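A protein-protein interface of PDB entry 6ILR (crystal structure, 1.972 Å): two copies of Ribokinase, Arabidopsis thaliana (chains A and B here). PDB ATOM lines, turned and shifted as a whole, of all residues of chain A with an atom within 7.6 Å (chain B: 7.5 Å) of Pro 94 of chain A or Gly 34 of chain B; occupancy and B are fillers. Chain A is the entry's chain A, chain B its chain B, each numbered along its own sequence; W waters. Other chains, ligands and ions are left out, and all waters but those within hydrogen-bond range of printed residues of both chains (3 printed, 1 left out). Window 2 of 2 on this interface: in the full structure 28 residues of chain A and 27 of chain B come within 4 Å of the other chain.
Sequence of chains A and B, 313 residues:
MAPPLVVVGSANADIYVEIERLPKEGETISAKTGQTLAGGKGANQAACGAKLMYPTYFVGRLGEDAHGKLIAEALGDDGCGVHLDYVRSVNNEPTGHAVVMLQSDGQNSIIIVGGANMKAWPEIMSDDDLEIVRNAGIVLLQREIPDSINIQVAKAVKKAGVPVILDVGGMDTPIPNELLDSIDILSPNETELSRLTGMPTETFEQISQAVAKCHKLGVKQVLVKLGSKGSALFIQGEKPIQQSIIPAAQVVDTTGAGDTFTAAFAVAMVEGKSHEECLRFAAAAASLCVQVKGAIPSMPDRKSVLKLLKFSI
The backbone NH (N) of His 67 of chain A sits close to the side-chain carboxylate (OD1) of Asp 65 of chain A (3.5 Å).
O of Thr 95 of chain A sits at hydrogen-bond distance from ND1 of His 97 of chain A, 2.8 Å away.
The backbone carbonyl oxygen of His 97 of chain A sits at hydrogen-bond distance from the backbone NH of Val 113 of chain A, 2.8 Å away.
The backbone NH (N) of Ala 116 of chain A lies within hydrogen-bond range of the backbone carbonyl oxygen (O) of Pro 94 of chain A, at 2.8 Å.
Ile 15 of chain B touches His 67 of chain A (CD1 to CE1, 3.6 Å).
His 67 of chain A touches Thr 36 of chain B.
Gly 34 of chain B touches Pro 94 of chain A.
CG1 of Val 17 of chain B touches NE2 of His 97 of chain A, 3.8 Å away.
CG1 of Val 17 of chain B touches CG2 of Val 113 of chain A (3.8 Å).
CB of Ala 31 of chain B touches CG2 of Val 113 of chain A (3.6 Å).
Water W3 lies within hydrogen-bond range of the side-chain hydroxyl (OG1) of Thr 36 of chain B (2.8 Å) and a ring nitrogen (NE2) of His 97 of chain A (3.2 Å).
Water W1 bridges OE1 of Glu 93 of chain A (2.8 Å) and OG1 of Thr 33 of chain B (3.0 Å).
Water W2 lies within hydrogen-bond range of the backbone NH of Thr 36 of chain B (3.1 Å) and the side-chain carboxylate of Asp 65 of chain A (3.1 Å).
Hydrophobic or aromatic side chains of chain A that line the printed part of chain B: His 67, Pro 94, His 97 and Val 113.
Hydrophobic or aromatic side chains of chain B within 4 Å of the printed part of chain A: Ile 15, Val 17 and Ala 31.
Among the printed residues, 6 pairs touch across the chains.
Of chain B, only Gly 34 comes within 4 Å of Pro 94 of chain A.
Of the printed residues of chain A, Ile 15 of chain B touches His 67.
Of the printed residues of chain A, Ala 31 of chain B touches Val 113 (3.6 Å).
Gly 34 of chain B touches just one residue of chain A: Pro 94.
The nearest residue of chain B that does not touch Pro 94 of chain A is Thr 33 of chain B (4.2 Å).
The nearest residue of chain A that does not touch Gly 34 of chain B is Val 113 of chain A (4.1 Å).
No position is printed for both chains.
Of the 6 pairs that touch across the chains among the printed residues, none has its exchanged pair printed and touching as well.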
ATOM      1  N   ALA A  11       5.470   3.928 -18.872  1.00  0.00           N
ATOM      2  CA  ALA A  11       4.618   3.815 -17.696  1.00  0.00           C
ATOM      3  C   ALA A  11       3.999   2.421 -17.702  1.00  0.00           C
ATOM      4  O   ALA A  11       3.454   1.973 -18.716  1.00  0.00           O
ATOM      5  CB  ALA A  11       3.560   4.885 -17.679  1.00  0.00           C
ATOM      6  N   ARG A  61       2.847   7.363 -23.142  1.00  0.00           N
ATOM      7  CA  ARG A  61       1.629   6.911 -23.799  1.00  0.00           C
ATOM      8  C   ARG A  61       0.956   5.857 -22.944  1.00  0.00           C
ATOM      9  O   ARG A  61       1.615   4.912 -22.497  1.00  0.00           O
ATOM     10  CB  ARG A  61       1.937   6.351 -25.189  1.00  0.00           C
ATOM     11  CG  ARG A  61       2.403   7.399 -26.199  1.00  0.00           C
ATOM     12  CD  ARG A  61       1.330   8.434 -26.454  1.00  0.00           C
ATOM     13  NE  ARG A  61       1.728   9.418 -27.460  1.00  0.00           N
ATOM     14  CZ  ARG A  61       2.307  10.584 -27.183  1.00  0.00           C
ATOM     15  NH1 ARG A  61       2.570  10.924 -25.925  1.00  0.00           N
ATOM     16  NH2 ARG A  61       2.628  11.410 -28.169  1.00  0.00           N
ATOM     17  N   LEU A  62      -0.351   6.027 -22.732  1.00  0.00           N
ATOM     18  CA  LEU A  62      -1.168   5.098 -21.954  1.00  0.00           C
ATOM     19  C   LEU A  62      -2.287   4.506 -22.799  1.00  0.00           C
ATOM     20  O   LEU A  62      -2.606   5.030 -23.865  1.00  0.00           O
ATOM     21  CB  LEU A  62      -1.793   5.804 -20.748  1.00  0.00           C
ATOM     22  CG  LEU A  62      -0.839   6.538 -19.817  1.00  0.00           C
ATOM     23  CD1 LEU A  62      -1.610   7.241 -18.695  1.00  0.00           C
ATOM     24  CD2 LEU A  62       0.185   5.549 -19.272  1.00  0.00           C
ATOM     25  N   GLY A  63      -2.896   3.433 -22.304  1.00  0.00           N
ATOM     26  CA  GLY A  63      -4.138   2.947 -22.869  1.00  0.00           C
ATOM     27  C   GLY A  63      -5.305   3.627 -22.174  1.00  0.00           C
ATOM     28  O   GLY A  63      -5.159   4.159 -21.070  1.00  0.00           O
ATOM     29  N   GLU A  64      -6.467   3.633 -22.817  1.00  0.00           N
ATOM     30  CA  GLU A  64      -7.671   4.131 -22.167  1.00  0.00           C
ATOM     31  C   GLU A  64      -8.292   2.987 -21.381  1.00  0.00           C
ATOM     32  O   GLU A  64      -9.283   2.400 -21.813  1.00  0.00           O
ATOM     33  CB  GLU A  64      -8.659   4.696 -23.190  1.00  0.00           C
ATOM     34  CG  GLU A  64      -8.178   5.972 -23.854  1.00  0.00           C
ATOM     35  CD  GLU A  64      -9.114   6.465 -24.944  1.00  0.00           C
ATOM     36  OE1 GLU A  64     -10.134   5.793 -25.204  1.00  0.00           O
ATOM     37  OE2 GLU A  64      -8.824   7.522 -25.544  1.00  0.00           O
ATOM     38  N   ASP A  65      -7.684   2.670 -20.238  1.00  0.00           N
ATOM     39  CA  ASP A  65      -8.048   1.502 -19.437  1.00  0.00           C
ATOM     40  C   ASP A  65      -7.732   1.769 -17.973  1.00  0.00           C
ATOM     41  O   ASP A  65      -7.174   2.811 -17.653  1.00  0.00           O
ATOM     42  CB  ASP A  65      -7.303   0.251 -19.917  1.00  0.00           C
ATOM     43  CG  ASP A  65      -5.785   0.450 -19.975  1.00  0.00           C
ATOM     44  OD1 ASP A  65      -5.265   1.357 -19.295  1.00  0.00           O
ATOM     45  OD2 ASP A  65      -5.107  -0.320 -20.690  1.00  0.00           O
ATOM     46  N   HIS A  67      -5.497   0.514 -15.925  1.00  0.00           N
ATOM     47  CA  HIS A  67      -4.079   0.676 -15.597  1.00  0.00           C
ATOM     48  C   HIS A  67      -3.587   2.080 -15.951  1.00  0.00           C
ATOM     49  O   HIS A  67      -2.695   2.623 -15.291  1.00  0.00           O
ATOM     50  CB  HIS A  67      -3.249  -0.390 -16.303  1.00  0.00           C
ATOM     51  CG  HIS A  67      -3.556  -1.777 -15.837  1.00  0.00           C
ATOM     52  ND1 HIS A  67      -3.351  -2.892 -16.624  1.00  0.00           N
ATOM     53  CD2 HIS A  67      -4.060  -2.228 -14.665  1.00  0.00           C
ATOM     54  CE1 HIS A  67      -3.725  -3.970 -15.952  1.00  0.00           C
ATOM     55  NE2 HIS A  67      -4.156  -3.596 -14.766  1.00  0.00           N
ATOM     56  N   GLY A  68      -4.158   2.664 -16.997  1.00  0.00           N
ATOM     57  CA  GLY A  68      -3.838   4.037 -17.345  1.00  0.00           C
ATOM     58  C   GLY A  68      -4.281   5.003 -16.260  1.00  0.00           C
ATOM     59  O   GLY A  68      -3.556   5.929 -15.892  1.00  0.00           O
ATOM     60  N   VAL A  90      -4.547   6.169 -25.739  1.00  0.00           N
ATOM     61  CA  VAL A  90      -5.093   5.634 -26.979  1.00  0.00           C
ATOM     62  C   VAL A  90      -6.100   4.521 -26.685  1.00  0.00           C
ATOM     63  O   VAL A  90      -6.047   3.892 -25.631  1.00  0.00           O
ATOM     64  CB  VAL A  90      -3.984   5.096 -27.892  1.00  0.00           C
ATOM     65  CG1 VAL A  90      -2.987   6.202 -28.218  1.00  0.00           C
ATOM     66  CG2 VAL A  90      -3.286   3.917 -27.239  1.00  0.00           C
ATOM     67  N   ASN A  91      -7.019   4.273 -27.613  1.00  0.00           N
ATOM     68  CA  ASN A  91      -8.054   3.274 -27.368  1.00  0.00           C
ATOM     69  C   ASN A  91      -7.780   1.943 -28.055  1.00  0.00           C
ATOM     70  O   ASN A  91      -8.573   1.013 -27.943  1.00  0.00           O
ATOM     71  CB  ASN A  91      -9.428   3.810 -27.794  1.00  0.00           C
ATOM     72  CG  ASN A  91      -9.443   4.348 -29.218  1.00  0.00           C
ATOM     73  OD1 ASN A  91      -8.720   3.870 -30.096  1.00  0.00           O
ATOM     74  ND2 ASN A  91     -10.278   5.355 -29.452  1.00  0.00           N
ATOM     75  N   ASN A  92      -6.656   1.840 -28.756  1.00  0.00           N
ATOM     76  CA  ASN A  92      -6.357   0.603 -29.483  1.00  0.00           C
ATOM     77  C   ASN A  92      -5.153  -0.147 -28.924  1.00  0.00           C
ATOM     78  O   ASN A  92      -4.695  -1.124 -29.511  1.00  0.00           O
ATOM     79  CB  ASN A  92      -6.138   0.899 -30.966  1.00  0.00           C
ATOM     80  CG  ASN A  92      -4.985   1.841 -31.204  1.00  0.00           C
ATOM     81  OD1 ASN A  92      -4.592   2.594 -30.313  1.00  0.00           O
ATOM     82  ND2 ASN A  92      -4.435   1.812 -32.413  1.00  0.00           N
ATOM     83  N   GLU A  93      -4.642   0.315 -27.785  1.00  0.00           N
ATOM     84  CA  GLU A  93      -3.537  -0.356 -27.114  1.00  0.00           C
ATOM     85  C   GLU A  93      -3.756  -0.328 -25.614  1.00  0.00           C
ATOM     86  O   GLU A  93      -4.265   0.647 -25.084  1.00  0.00           O
ATOM     87  CB  GLU A  93      -2.193   0.307 -27.452  1.00  0.00           C
ATOM     88  CG  GLU A  93      -1.743   0.127 -28.891  1.00  0.00           C
ATOM     89  CD  GLU A  93      -1.436  -1.324 -29.232  1.00  0.00           C
ATOM     90  OE1 GLU A  93      -1.134  -2.111 -28.307  1.00  0.00           O
ATOM     91  OE2 GLU A  93      -1.497  -1.675 -30.428  1.00  0.00           O
ATOM     92  N   PRO A  94      -3.367  -1.404 -24.927  1.00  0.00           N
ATOM     93  CA  PRO A  94      -3.421  -1.399 -23.464  1.00  0.00           C
ATOM     94  C   PRO A  94      -2.245  -0.632 -22.876  1.00  0.00           C
ATOM     95  O   PRO A  94      -1.161  -0.587 -23.477  1.00  0.00           O
ATOM     96  CB  PRO A  94      -3.325  -2.880 -23.113  1.00  0.00           C
ATOM     97  CG  PRO A  94      -2.420  -3.433 -24.222  1.00  0.00           C
ATOM     98  CD  PRO A  94      -2.830  -2.669 -25.464  1.00  0.00           C
ATOM     99  N   THR A  95      -2.466  -0.025 -21.717  1.00  0.00           N
ATOM    100  CA  THR A  95      -1.372   0.479 -20.902  1.00  0.00           C
ATOM    101  C   THR A  95      -0.357  -0.635 -20.710  1.00  0.00           C
ATOM    102  O   THR A  95      -0.728  -1.795 -20.522  1.00  0.00           O
ATOM    103  CB  THR A  95      -1.877   0.980 -19.546  1.00  0.00           C
ATOM    104  OG1 THR A  95      -2.754   2.092 -19.754  1.00  0.00           O
ATOM    105  CG2 THR A  95      -0.724   1.427 -18.652  1.00  0.00           C
ATOM    106  N   GLY A  96       0.924  -0.297 -20.795  1.00  0.00           N
ATOM    107  CA  GLY A  96       1.962  -1.284 -20.584  1.00  0.00           C
ATOM    108  C   GLY A  96       1.868  -1.890 -19.197  1.00  0.00           C
ATOM    109  O   GLY A  96       1.505  -1.208 -18.237  1.00  0.00           O
ATOM    110  N   HIS A  97       2.189  -3.176 -19.087  1.00  0.00           N
ATOM    111  CA  HIS A  97       2.154  -3.847 -17.792  1.00  0.00           C
ATOM    112  C   HIS A  97       3.046  -5.083 -17.730  1.00  0.00           C
ATOM    113  O   HIS A  97       3.443  -5.646 -18.754  1.00  0.00           O
ATOM    114  CB  HIS A  97       0.705  -4.220 -17.407  1.00  0.00           C
ATOM    115  CG  HIS A  97      -0.042  -4.981 -18.456  1.00  0.00           C
ATOM    116  ND1 HIS A  97      -0.472  -4.407 -19.636  1.00  0.00           N
ATOM    117  CD2 HIS A  97      -0.496  -6.261 -18.482  1.00  0.00           C
ATOM    118  CE1 HIS A  97      -1.123  -5.305 -20.353  1.00  0.00           C
ATOM    119  NE2 HIS A  97      -1.150  -6.438 -19.674  1.00  0.00           N
ATOM    120  N   VAL A 113       4.240  -6.966 -21.048  1.00  0.00           N
ATOM    121  CA  VAL A 113       3.412  -6.471 -22.148  1.00  0.00           C
ATOM    122  C   VAL A 113       3.801  -5.035 -22.500  1.00  0.00           C
ATOM    123  O   VAL A 113       3.560  -4.109 -21.723  1.00  0.00           O
ATOM    124  CB  VAL A 113       1.913  -6.520 -21.807  1.00  0.00           C
ATOM    125  CG1 VAL A 113       1.096  -5.996 -22.978  1.00  0.00           C
ATOM    126  CG2 VAL A 113       1.498  -7.936 -21.452  1.00  0.00           C
ATOM    127  N   GLY A 114       4.409  -4.860 -23.669  1.00  0.00           N
ATOM    128  CA  GLY A 114       4.839  -3.549 -24.114  1.00  0.00           C
ATOM    129  C   GLY A 114       3.689  -2.569 -24.151  1.00  0.00           C
ATOM    130  O   GLY A 114       3.778  -1.473 -23.596  1.00  0.00           O
ATOM    131  N   GLY A 115       2.601  -2.974 -24.795  1.00  0.00           N
ATOM    132  CA  GLY A 115       1.405  -2.159 -24.858  1.00  0.00           C
ATOM    133  C   GLY A 115       1.695  -0.796 -25.445  1.00  0.00           C
ATOM    134  O   GLY A 115       2.494  -0.671 -26.368  1.00  0.00           O
ATOM    135  N   ALA A 116       1.069   0.231 -24.882  1.00  0.00           N
ATOM    136  CA  ALA A 116       1.178   1.577 -25.413  1.00  0.00           C
ATOM    137  C   ALA A 116       2.614   2.129 -25.368  1.00  0.00           C
ATOM    138  O   ALA A 116       2.966   2.976 -26.192  1.00  0.00           O
ATOM    139  CB  ALA A 116       0.225   2.510 -24.664  1.00  0.00           C
ATOM    140  N   ASN A 117       3.436   1.659 -24.424  1.00  0.00           N
ATOM    141  CA  ASN A 117       4.827   2.131 -24.326  1.00  0.00           C
ATOM    142  C   ASN A 117       5.575   1.912 -25.629  1.00  0.00           C
ATOM    143  O   ASN A 117       6.373   2.751 -26.056  1.00  0.00           O
ATOM    144  CB  ASN A 117       5.577   1.421 -23.194  1.00  0.00           C
ATOM    145  CG  ASN A 117       5.055   1.791 -21.827  1.00  0.00           C
ATOM    146  OD1 ASN A 117       4.820   2.969 -21.529  1.00  0.00           O
ATOM    147  ND2 ASN A 117       4.849   0.784 -20.988  1.00  0.00           N
ATOM    148  N   MET A 118       5.296   0.775 -26.258  1.00  0.00           N
ATOM    149  CA  MET A 118       5.971   0.380 -27.489  1.00  0.00           C
ATOM    150  C   MET A 118       5.148   0.638 -28.742  1.00  0.00           C
ATOM    151  O   MET A 118       5.700   0.754 -29.833  1.00  0.00           O
ATOM    152  CB  MET A 118       6.344  -1.105 -27.431  1.00  0.00           C
ATOM    153  CG  MET A 118       7.354  -1.427 -26.348  1.00  0.00           C
ATOM    154  SD  MET A 118       8.912  -0.547 -26.627  1.00  0.00           S
ATOM    155  CE  MET A 118       9.409  -1.210 -28.217  1.00  0.00           C
ATOM    156  N   LYS A 119       3.831   0.736 -28.601  1.00  0.00           N
ATOM    157  CA  LYS A 119       2.982   0.713 -29.788  1.00  0.00           C
ATOM    158  C   LYS A 119       2.068   1.916 -29.991  1.00  0.00           C
ATOM    159  O   LYS A 119       1.400   1.998 -31.019  1.00  0.00           O
ATOM    160  CB  LYS A 119       2.123  -0.553 -29.770  1.00  0.00           C
ATOM    161  CG  LYS A 119       2.914  -1.850 -29.923  1.00  0.00           C
ATOM    162  CD  LYS A 119       1.967  -3.040 -29.927  1.00  0.00           C
ATOM    163  CE  LYS A 119       2.672  -4.333 -30.285  1.00  0.00           C
ATOM    164  NZ  LYS A 119       3.761  -4.645 -29.328  1.00  0.00           N
ATOM    165  N   ALA A 120       2.024   2.849 -29.043  1.00  0.00           N
ATOM    166  CA  ALA A 120       1.065   3.960 -29.156  1.00  0.00           C
ATOM    167  C   ALA A 120       1.710   5.275 -29.585  1.00  0.00           C
ATOM    168  O   ALA A 120       1.036   6.291 -29.727  1.00  0.00           O
ATOM    169  CB  ALA A 120       0.328   4.154 -27.841  1.00  0.00           C
ATOM    170  N   ILE B  15      -7.291  -9.772 -16.195  1.00  0.00           N
ATOM    171  CA  ILE B  15      -6.073  -9.367 -16.889  1.00  0.00           C
ATOM    172  C   ILE B  15      -5.664 -10.424 -17.912  1.00  0.00           C
ATOM    173  O   ILE B  15      -5.026 -11.418 -17.565  1.00  0.00           O
ATOM    174  CB  ILE B  15      -4.907  -9.158 -15.915  1.00  0.00           C
ATOM    175  CG1 ILE B  15      -5.337  -8.339 -14.692  1.00  0.00           C
ATOM    176  CG2 ILE B  15      -3.728  -8.515 -16.634  1.00  0.00           C
ATOM    177  CD1 ILE B  15      -5.629  -6.914 -15.003  1.00  0.00           C
ATOM    178  N   TYR B  16      -6.043 -10.210 -19.167  1.00  0.00           N
ATOM    179  CA  TYR B  16      -5.717 -11.147 -20.239  1.00  0.00           C
ATOM    180  C   TYR B  16      -4.389 -10.801 -20.878  1.00  0.00           C
ATOM    181  O   TYR B  16      -4.169  -9.652 -21.241  1.00  0.00           O
ATOM    182  CB  TYR B  16      -6.800 -11.140 -21.315  1.00  0.00           C
ATOM    183  CG  TYR B  16      -8.137 -11.632 -20.837  1.00  0.00           C
ATOM    184  CD1 TYR B  16      -8.403 -12.991 -20.749  1.00  0.00           C
ATOM    185  CD2 TYR B  16      -9.138 -10.741 -20.481  1.00  0.00           C
ATOM    186  CE1 TYR B  16      -9.629 -13.452 -20.309  1.00  0.00           C
ATOM    187  CE2 TYR B  16     -10.372 -11.189 -20.045  1.00  0.00           C
ATOM    188  CZ  TYR B  16     -10.611 -12.546 -19.959  1.00  0.00           C
ATOM    189  OH  TYR B  16     -11.837 -12.996 -19.520  1.00  0.00           O
ATOM    190  N   VAL B  17      -3.513 -11.793 -21.025  1.00  0.00           N
ATOM    191  CA  VAL B  17      -2.268 -11.603 -21.762  1.00  0.00           C
ATOM    192  C   VAL B  17      -2.065 -12.720 -22.792  1.00  0.00           C
ATOM    193  O   VAL B  17      -2.248 -13.901 -22.492  1.00  0.00           O
ATOM    194  CB  VAL B  17      -1.051 -11.536 -20.818  1.00  0.00           C
ATOM    195  CG1 VAL B  17      -1.092 -10.256 -19.990  1.00  0.00           C
ATOM    196  CG2 VAL B  17      -0.990 -12.758 -19.914  1.00  0.00           C
ATOM    197  N   GLU B  18      -1.709 -12.334 -24.013  1.00  0.00           N
ATOM    198  CA  GLU B  18      -1.431 -13.295 -25.079  1.00  0.00           C
ATOM    199  C   GLU B  18       0.045 -13.658 -25.099  1.00  0.00           C
ATOM    200  O   GLU B  18       0.895 -12.838 -25.450  1.00  0.00           O
ATOM    201  CB  GLU B  18      -1.844 -12.737 -26.443  1.00  0.00           C
ATOM    202  CG  GLU B  18      -3.326 -12.844 -26.741  1.00  0.00           C
ATOM    203  CD  GLU B  18      -3.686 -12.332 -28.124  1.00  0.00           C
ATOM    204  OE1 GLU B  18      -2.882 -12.527 -29.064  1.00  0.00           O
ATOM    205  OE2 GLU B  18      -4.775 -11.731 -28.268  1.00  0.00           O
ATOM    206  N   ALA B  31       4.893 -10.779 -23.897  1.00  0.00           N
ATOM    207  CA  ALA B  31       3.584 -11.111 -24.436  1.00  0.00           C
ATOM    208  C   ALA B  31       3.316 -10.322 -25.712  1.00  0.00           C
ATOM    209  O   ALA B  31       3.812  -9.210 -25.882  1.00  0.00           O
ATOM    210  CB  ALA B  31       2.500 -10.840 -23.406  1.00  0.00           C
ATOM    211  N   LYS B  32       2.525 -10.905 -26.604  1.00  0.00           N
ATOM    212  CA  LYS B  32       2.151 -10.247 -27.849  1.00  0.00           C
ATOM    213  C   LYS B  32       1.325  -9.006 -27.554  1.00  0.00           C
ATOM    214  O   LYS B  32       1.616  -7.915 -28.039  1.00  0.00           O
ATOM    215  CB  LYS B  32       1.366 -11.207 -28.747  1.00  0.00           C
ATOM    216  CG  LYS B  32       0.920 -10.612 -30.084  1.00  0.00           C
ATOM    217  CD  LYS B  32       0.008 -11.564 -30.864  1.00  0.00           C
ATOM    218  CE  LYS B  32       0.173 -13.022 -30.436  1.00  0.00           C
ATOM    219  NZ  LYS B  32      -0.222 -13.971 -31.520  1.00  0.00           N
ATOM    220  N   THR B  33       0.286  -9.185 -26.748  1.00  0.00           N
ATOM    221  CA  THR B  33      -0.562  -8.075 -26.356  1.00  0.00           C
ATOM    222  C   THR B  33      -1.311  -8.412 -25.072  1.00  0.00           C
ATOM    223  O   THR B  33      -1.018  -9.413 -24.406  1.00  0.00           O
ATOM    224  CB  THR B  33      -1.559  -7.708 -27.470  1.00  0.00           C
ATOM    225  OG1 THR B  33      -2.359  -6.593 -27.057  1.00  0.00           O
ATOM    226  CG2 THR B  33      -2.455  -8.886 -27.796  1.00  0.00           C
ATOM    227  N   GLY B  34      -2.272  -7.567 -24.720  1.00  0.00           N
ATOM    228  CA  GLY B  34      -3.024  -7.756 -23.499  1.00  0.00           C
ATOM    229  C   GLY B  34      -4.279  -6.917 -23.480  1.00  0.00           C
ATOM    230  O   GLY B  34      -4.463  -6.015 -24.304  1.00  0.00           O
ATOM    231  N   GLN B  35      -5.158  -7.230 -22.535  1.00  0.00           N
ATOM    232  CA  GLN B  35      -6.347  -6.429 -22.307  1.00  0.00           C
ATOM    233  C   GLN B  35      -6.842  -6.664 -20.881  1.00  0.00           C
ATOM    234  O   GLN B  35      -6.695  -7.760 -20.335  1.00  0.00           O
ATOM    235  CB  GLN B  35      -7.427  -6.760 -23.334  1.00  0.00           C
ATOM    236  CG  GLN B  35      -8.539  -5.734 -23.407  1.00  0.00           C
ATOM    237  CD  GLN B  35      -9.487  -5.993 -24.557  1.00  0.00           C
ATOM    238  OE1 GLN B  35      -9.434  -7.048 -25.189  1.00  0.00           O
ATOM    239  NE2 GLN B  35     -10.362  -5.031 -24.839  1.00  0.00           N
ATOM    240  N   THR B  36      -7.388  -5.620 -20.269  1.00  0.00           N
ATOM    241  CA  THR B  36      -7.982  -5.737 -18.942  1.00  0.00           C
ATOM    242  C   THR B  36      -9.461  -5.432 -19.030  1.00  0.00           C
ATOM    243  O   THR B  36      -9.840  -4.370 -19.516  1.00  0.00           O
ATOM    244  CB  THR B  36      -7.335  -4.789 -17.930  1.00  0.00           C
ATOM    245  OG1 THR B  36      -5.988  -5.204 -17.690  1.00  0.00           O
ATOM    246  CG2 THR B  36      -8.102  -4.822 -16.613  1.00  0.00           C
HETATM  247  O   HOH W   1      -0.179  -4.663 -27.601  1.00  0.00           O
HETATM  248  O   HOH W   2      -6.479  -2.956 -21.484  1.00  0.00           O
HETATM  249  O   HOH W   3      -4.039  -4.983 -19.693  1.00  0.00           O
